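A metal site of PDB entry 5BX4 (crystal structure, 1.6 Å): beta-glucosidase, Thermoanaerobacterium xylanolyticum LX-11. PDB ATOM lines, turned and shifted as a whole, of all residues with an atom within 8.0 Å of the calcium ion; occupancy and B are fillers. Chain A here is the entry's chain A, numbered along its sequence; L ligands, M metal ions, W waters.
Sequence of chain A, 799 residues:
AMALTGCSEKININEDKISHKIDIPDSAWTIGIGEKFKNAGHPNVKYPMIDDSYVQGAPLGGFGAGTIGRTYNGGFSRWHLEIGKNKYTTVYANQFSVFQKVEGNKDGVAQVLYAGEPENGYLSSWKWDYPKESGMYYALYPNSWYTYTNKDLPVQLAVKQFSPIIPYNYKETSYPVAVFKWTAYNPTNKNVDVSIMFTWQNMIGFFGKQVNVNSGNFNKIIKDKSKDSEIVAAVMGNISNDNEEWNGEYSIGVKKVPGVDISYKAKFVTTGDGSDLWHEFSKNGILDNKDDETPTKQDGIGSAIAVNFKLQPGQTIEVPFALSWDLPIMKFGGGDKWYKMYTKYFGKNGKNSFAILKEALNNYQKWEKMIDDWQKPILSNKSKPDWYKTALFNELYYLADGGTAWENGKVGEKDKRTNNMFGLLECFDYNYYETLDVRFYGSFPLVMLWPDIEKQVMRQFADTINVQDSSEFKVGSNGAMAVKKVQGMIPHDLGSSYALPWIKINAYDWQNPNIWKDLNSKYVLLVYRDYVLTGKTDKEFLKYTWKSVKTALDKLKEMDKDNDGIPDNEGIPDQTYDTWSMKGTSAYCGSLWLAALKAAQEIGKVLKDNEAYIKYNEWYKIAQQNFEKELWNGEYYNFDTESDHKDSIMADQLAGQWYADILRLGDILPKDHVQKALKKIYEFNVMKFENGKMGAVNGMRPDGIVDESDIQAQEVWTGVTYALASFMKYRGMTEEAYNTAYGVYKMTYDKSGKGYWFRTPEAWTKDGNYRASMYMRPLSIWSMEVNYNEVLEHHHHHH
N of Lys 561 sits close to OD1 of Asp 568, at 3.0 Å. The backbone NH (N) of Asp 568 is in hydrogen-bond range of the backbone carbonyl oxygen (O) of Met 559, at 2.9 Å. OG1 of Thr 585 is in hydrogen-bond range of OD2 of Asp 564 (3.0 Å). OE2 of Glu 630 lies close to OD2 of Asp 564 (2.6 Å). O of Asp 564 is in hydrogen-bond range of ND2 of Asn 626 (2.8 Å). The side-chain carboxylate (OD1) of Asp 560 sits close to the backbone NH (N) of Asn 563, 3.2 Å away. The side-chain carboxylate (OD2) of Asp 560 is in hydrogen-bond range of the backbone NH (N) of Gly 565 (2.8 Å).
Within 4 Å of the calcium ion: Asp 560, Asp 562, Asp 564, Ile 566 and Asp 568. The nearest printed residue that does not touch the calcium ion is Pro 567 (4.3 Å).
The calcium ion is bound by the side-chain carboxylate (OD1) of Asp 568 (2.2 Å), the side-chain carboxylate (OD1) of Asp 564 (2.3 Å), water W1 (2.3 Å), the backbone carbonyl oxygen (O) of Ile 566 (2.4 Å), the side-chain carboxylate (OD1) of Asp 562 (2.5 Å), the side-chain carboxylate (OD1) of Asp 560 (2.5 Å) and an oxygen (O3) of the ligand (2.8 Å).
Water W1 bridges the side-chain hydroxyl of Thr 585 (2.7 Å) and the backbone carbonyl oxygen of Pro 567 (3.0 Å).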
ATOM      1  N   LYS A 557      -4.535  -8.725  19.570  1.00  0.00           N
ATOM      2  CA  LYS A 557      -3.518  -9.509  20.285  1.00  0.00           C
ATOM      3  C   LYS A 557      -2.156  -9.444  19.565  1.00  0.00           C
ATOM      4  O   LYS A 557      -1.112  -9.383  20.217  1.00  0.00           O
ATOM      5  CB  LYS A 557      -3.992 -10.954  20.416  1.00  0.00           C
ATOM      6  CG  LYS A 557      -3.081 -11.883  21.199  1.00  0.00           C
ATOM      7  CD  LYS A 557      -2.791 -11.337  22.586  1.00  0.00           C
ATOM      8  CE  LYS A 557      -2.620 -12.436  23.613  1.00  0.00           C
ATOM      9  NZ  LYS A 557      -1.416 -13.257  23.368  1.00  0.00           N
ATOM     10  N   MET A 559      -0.830  -6.947  18.304  1.00  0.00           N
ATOM     11  CA  MET A 559      -0.169  -5.690  18.651  1.00  0.00           C
ATOM     12  C   MET A 559       0.496  -5.706  20.030  1.00  0.00           C
ATOM     13  O   MET A 559       1.028  -4.681  20.484  1.00  0.00           O
ATOM     14  CB  MET A 559      -1.162  -4.528  18.533  1.00  0.00           C
ATOM     15  CG  MET A 559      -1.614  -4.319  17.109  1.00  0.00           C
ATOM     16  SD  MET A 559      -2.979  -3.163  16.974  1.00  0.00           S
ATOM     17  CE  MET A 559      -3.378  -3.358  15.240  1.00  0.00           C
ATOM     18  N   ASP A 560       0.492  -6.849  20.692  1.00  0.00           N
ATOM     19  CA  ASP A 560       1.285  -7.050  21.893  1.00  0.00           C
ATOM     20  C   ASP A 560       2.733  -7.306  21.457  1.00  0.00           C
ATOM     21  O   ASP A 560       3.050  -8.374  20.968  1.00  0.00           O
ATOM     22  CB  ASP A 560       0.742  -8.254  22.660  1.00  0.00           C
ATOM     23  CG  ASP A 560       1.534  -8.575  23.911  1.00  0.00           C
ATOM     24  OD1 ASP A 560       2.301  -7.708  24.381  1.00  0.00           O
ATOM     25  OD2 ASP A 560       1.367  -9.686  24.430  1.00  0.00           O
ATOM     26  N   LYS A 561       3.604  -6.320  21.643  1.00  0.00           N
ATOM     27  CA  LYS A 561       4.987  -6.406  21.152  1.00  0.00           C
ATOM     28  C   LYS A 561       6.001  -6.968  22.167  1.00  0.00           C
ATOM     29  O   LYS A 561       7.167  -7.157  21.821  1.00  0.00           O
ATOM     30  CB  LYS A 561       5.453  -5.034  20.674  1.00  0.00           C
ATOM     31  CG  LYS A 561       4.757  -4.570  19.404  1.00  0.00           C
ATOM     32  CD  LYS A 561       5.304  -3.258  18.874  1.00  0.00           C
ATOM     33  CE  LYS A 561       5.109  -2.112  19.855  1.00  0.00           C
ATOM     34  NZ  LYS A 561       5.446  -0.792  19.245  1.00  0.00           N
ATOM     35  N   ASP A 562       5.586  -7.200  23.411  1.00  0.00           N
ATOM     36  CA  ASP A 562       6.503  -7.768  24.421  1.00  0.00           C
ATOM     37  C   ASP A 562       5.950  -8.968  25.174  1.00  0.00           C
ATOM     38  O   ASP A 562       6.477  -9.349  26.216  1.00  0.00           O
ATOM     39  CB  ASP A 562       6.899  -6.678  25.405  1.00  0.00           C
ATOM     40  CG  ASP A 562       5.720  -6.171  26.220  1.00  0.00           C
ATOM     41  OD1 ASP A 562       4.560  -6.440  25.832  1.00  0.00           O
ATOM     42  OD2 ASP A 562       5.966  -5.515  27.252  1.00  0.00           O
ATOM     43  N   ASN A 563       4.888  -9.568  24.645  1.00  0.00           N
ATOM     44  CA  ASN A 563       4.271 -10.749  25.230  1.00  0.00           C
ATOM     45  C   ASN A 563       3.883 -10.621  26.708  1.00  0.00           C
ATOM     46  O   ASN A 563       4.007 -11.574  27.480  1.00  0.00           O
ATOM     47  CB  ASN A 563       5.166 -11.984  25.008  1.00  0.00           C
ATOM     48  CG  ASN A 563       4.396 -13.300  25.102  1.00  0.00           C
ATOM     49  OD1 ASN A 563       3.170 -13.338  24.974  1.00  0.00           O
ATOM     50  ND2 ASN A 563       5.111 -14.386  25.332  1.00  0.00           N
ATOM     51  N   ASP A 564       3.401  -9.449  27.125  1.00  0.00           N
ATOM     52  CA  ASP A 564       2.753  -9.335  28.430  1.00  0.00           C
ATOM     53  C   ASP A 564       1.235  -9.633  28.337  1.00  0.00           C
ATOM     54  O   ASP A 564       0.520  -9.581  29.340  1.00  0.00           O
ATOM     55  CB  ASP A 564       3.039  -7.968  29.078  1.00  0.00           C
ATOM     56  CG  ASP A 564       2.227  -6.827  28.488  1.00  0.00           C
ATOM     57  OD1 ASP A 564       1.736  -6.956  27.347  1.00  0.00           O
ATOM     58  OD2 ASP A 564       2.109  -5.788  29.161  1.00  0.00           O
ATOM     59  N   GLY A 565       0.770  -9.968  27.132  1.00  0.00           N
ATOM     60  CA  GLY A 565      -0.617 -10.359  26.869  1.00  0.00           C
ATOM     61  C   GLY A 565      -1.538  -9.165  26.598  1.00  0.00           C
ATOM     62  O   GLY A 565      -2.756  -9.335  26.503  1.00  0.00           O
ATOM     63  N   ILE A 566      -0.955  -7.988  26.465  1.00  0.00           N
ATOM     64  CA  ILE A 566      -1.718  -6.748  26.302  1.00  0.00           C
ATOM     65  C   ILE A 566      -1.195  -5.994  25.078  1.00  0.00           C
ATOM     66  O   ILE A 566       0.027  -5.844  24.925  1.00  0.00           O
ATOM     67  CB  ILE A 566      -1.601  -5.851  27.555  1.00  0.00           C
ATOM     68  CG1 ILE A 566      -1.921  -6.658  28.822  1.00  0.00           C
ATOM     69  CG2 ILE A 566      -2.532  -4.638  27.455  1.00  0.00           C
ATOM     70  CD1 ILE A 566      -1.745  -5.907  30.103  1.00  0.00           C
ATOM     71  N   PRO A 567      -2.083  -5.524  24.196  1.00  0.00           N
ATOM     72  CA  PRO A 567      -1.593  -4.697  23.087  1.00  0.00           C
ATOM     73  C   PRO A 567      -0.817  -3.481  23.566  1.00  0.00           C
ATOM     74  O   PRO A 567      -1.151  -2.896  24.599  1.00  0.00           O
ATOM     75  CB  PRO A 567      -2.867  -4.274  22.348  1.00  0.00           C
ATOM     76  CG  PRO A 567      -4.001  -4.565  23.260  1.00  0.00           C
ATOM     77  CD  PRO A 567      -3.558  -5.620  24.219  1.00  0.00           C
ATOM     78  N   ASP A 568       0.249  -3.122  22.845  1.00  0.00           N
ATOM     79  CA  ASP A 568       1.104  -2.007  23.205  1.00  0.00           C
ATOM     80  C   ASP A 568       0.662  -0.741  22.497  1.00  0.00           C
ATOM     81  O   ASP A 568       0.649  -0.706  21.272  1.00  0.00           O
ATOM     82  CB  ASP A 568       2.560  -2.281  22.774  1.00  0.00           C
ATOM     83  CG  ASP A 568       3.271  -3.283  23.661  1.00  0.00           C
ATOM     84  OD1 ASP A 568       2.791  -4.442  23.798  1.00  0.00           O
ATOM     85  OD2 ASP A 568       4.333  -2.920  24.217  1.00  0.00           O
ATOM     86  N   ASN A 569       0.372   0.319  23.256  1.00  0.00           N
ATOM     87  CA  ASN A 569       0.229   1.641  22.652  1.00  0.00           C
ATOM     88  C   ASN A 569       1.607   2.077  22.140  1.00  0.00           C
ATOM     89  O   ASN A 569       2.634   1.767  22.751  1.00  0.00           O
ATOM     90  CB  ASN A 569      -0.335   2.657  23.648  1.00  0.00           C
ATOM     91  CG  ASN A 569      -1.780   2.357  24.026  1.00  0.00           C
ATOM     92  OD1 ASN A 569      -2.051   1.750  25.055  1.00  0.00           O
ATOM     93  ND2 ASN A 569      -2.715   2.788  23.190  1.00  0.00           N
ATOM     94  N   GLY A 584       3.073   1.774  25.637  1.00  0.00           N
ATOM     95  CA  GLY A 584       3.140   0.562  26.434  1.00  0.00           C
ATOM     96  C   GLY A 584       1.757   0.075  26.806  1.00  0.00           C
ATOM     97  O   GLY A 584       0.841   0.130  25.982  1.00  0.00           O
ATOM     98  N   THR A 585       1.602  -0.388  28.043  1.00  0.00           N
ATOM     99  CA  THR A 585       0.277  -0.769  28.561  1.00  0.00           C
ATOM    100  C   THR A 585      -0.364   0.483  29.142  1.00  0.00           C
ATOM    101  O   THR A 585       0.178   1.073  30.066  1.00  0.00           O
ATOM    102  CB  THR A 585       0.379  -1.861  29.631  1.00  0.00           C
ATOM    103  OG1 THR A 585       0.905  -3.051  29.040  1.00  0.00           O
ATOM    104  CG2 THR A 585      -0.984  -2.177  30.244  1.00  0.00           C
ATOM    105  N   ASN A 626      -0.906  -9.079  34.597  1.00  0.00           N
ATOM    106  CA  ASN A 626       0.097  -8.121  34.184  1.00  0.00           C
ATOM    107  C   ASN A 626      -0.351  -6.675  34.210  1.00  0.00           C
ATOM    108  O   ASN A 626       0.449  -5.786  34.465  1.00  0.00           O
ATOM    109  CB  ASN A 626       0.650  -8.490  32.809  1.00  0.00           C
ATOM    110  CG  ASN A 626       1.504  -9.735  32.861  1.00  0.00           C
ATOM    111  OD1 ASN A 626       2.046 -10.053  33.908  1.00  0.00           O
ATOM    112  ND2 ASN A 626       1.628 -10.435  31.747  1.00  0.00           N
ATOM    113  N   GLU A 630       1.691  -3.972  36.392  1.00  0.00           N
ATOM    114  CA  GLU A 630       2.330  -2.866  35.699  1.00  0.00           C
ATOM    115  C   GLU A 630       1.811  -1.487  36.115  1.00  0.00           C
ATOM    116  O   GLU A 630       2.555  -0.512  36.069  1.00  0.00           O
ATOM    117  CB  GLU A 630       2.125  -3.024  34.190  1.00  0.00           C
ATOM    118  CG  GLU A 630       2.923  -4.167  33.581  1.00  0.00           C
ATOM    119  CD  GLU A 630       2.404  -4.556  32.212  1.00  0.00           C
ATOM    120  OE1 GLU A 630       1.628  -3.768  31.615  1.00  0.00           O
ATOM    121  OE2 GLU A 630       2.750  -5.666  31.727  1.00  0.00           O
ATOM    122  N   THR A 641       2.629   2.707  31.030  1.00  0.00           N
ATOM    123  CA  THR A 641       3.922   2.204  31.523  1.00  0.00           C
ATOM    124  C   THR A 641       5.143   2.911  30.968  1.00  0.00           C
ATOM    125  O   THR A 641       6.228   2.767  31.537  1.00  0.00           O
ATOM    126  CB  THR A 641       4.062   0.697  31.223  1.00  0.00           C
ATOM    127  OG1 THR A 641       3.881   0.488  29.823  1.00  0.00           O
ATOM    128  CG2 THR A 641       3.047  -0.108  32.019  1.00  0.00           C
ATOM    129  N   GLU A 642       5.027   3.647  29.866  1.00  0.00           N
ATOM    130  CA  GLU A 642       6.217   4.201  29.200  1.00  0.00           C
ATOM    131  C   GLU A 642       6.252   5.705  28.856  1.00  0.00           C
ATOM    132  O   GLU A 642       7.286   6.204  28.419  1.00  0.00           O
ATOM    133  CB  GLU A 642       6.519   3.390  27.943  1.00  0.00           C
ATOM    134  CG  GLU A 642       6.808   1.923  28.201  1.00  0.00           C
ATOM    135  CD  GLU A 642       7.127   1.151  26.942  1.00  0.00           C
ATOM    136  OE1 GLU A 642       7.709   1.740  26.011  1.00  0.00           O
ATOM    137  OE2 GLU A 642       6.809  -0.055  26.869  1.00  0.00           O
HETATM  138  C1  LIG L   1       4.558  -3.239  29.990  1.00  0.00           C
HETATM  139  O1  LIG L   1       5.485  -3.310  31.070  1.00  0.00           O
HETATM  140  C2  LIG L   1       5.252  -2.664  28.756  1.00  0.00           C
HETATM  141  O2  LIG L   1       5.610  -1.300  28.994  1.00  0.00           O
HETATM  142  C3  LIG L   1       4.363  -2.731  27.519  1.00  0.00           C
HETATM  143  O3  LIG L   1       3.766  -4.016  27.350  1.00  0.00           O
HETATM  144 CA    CA M   1       2.266  -5.567  25.626  1.00  0.00          CA
HETATM  145  O   HOH W   1       1.186  -3.655  26.382  1.00  0.00           O
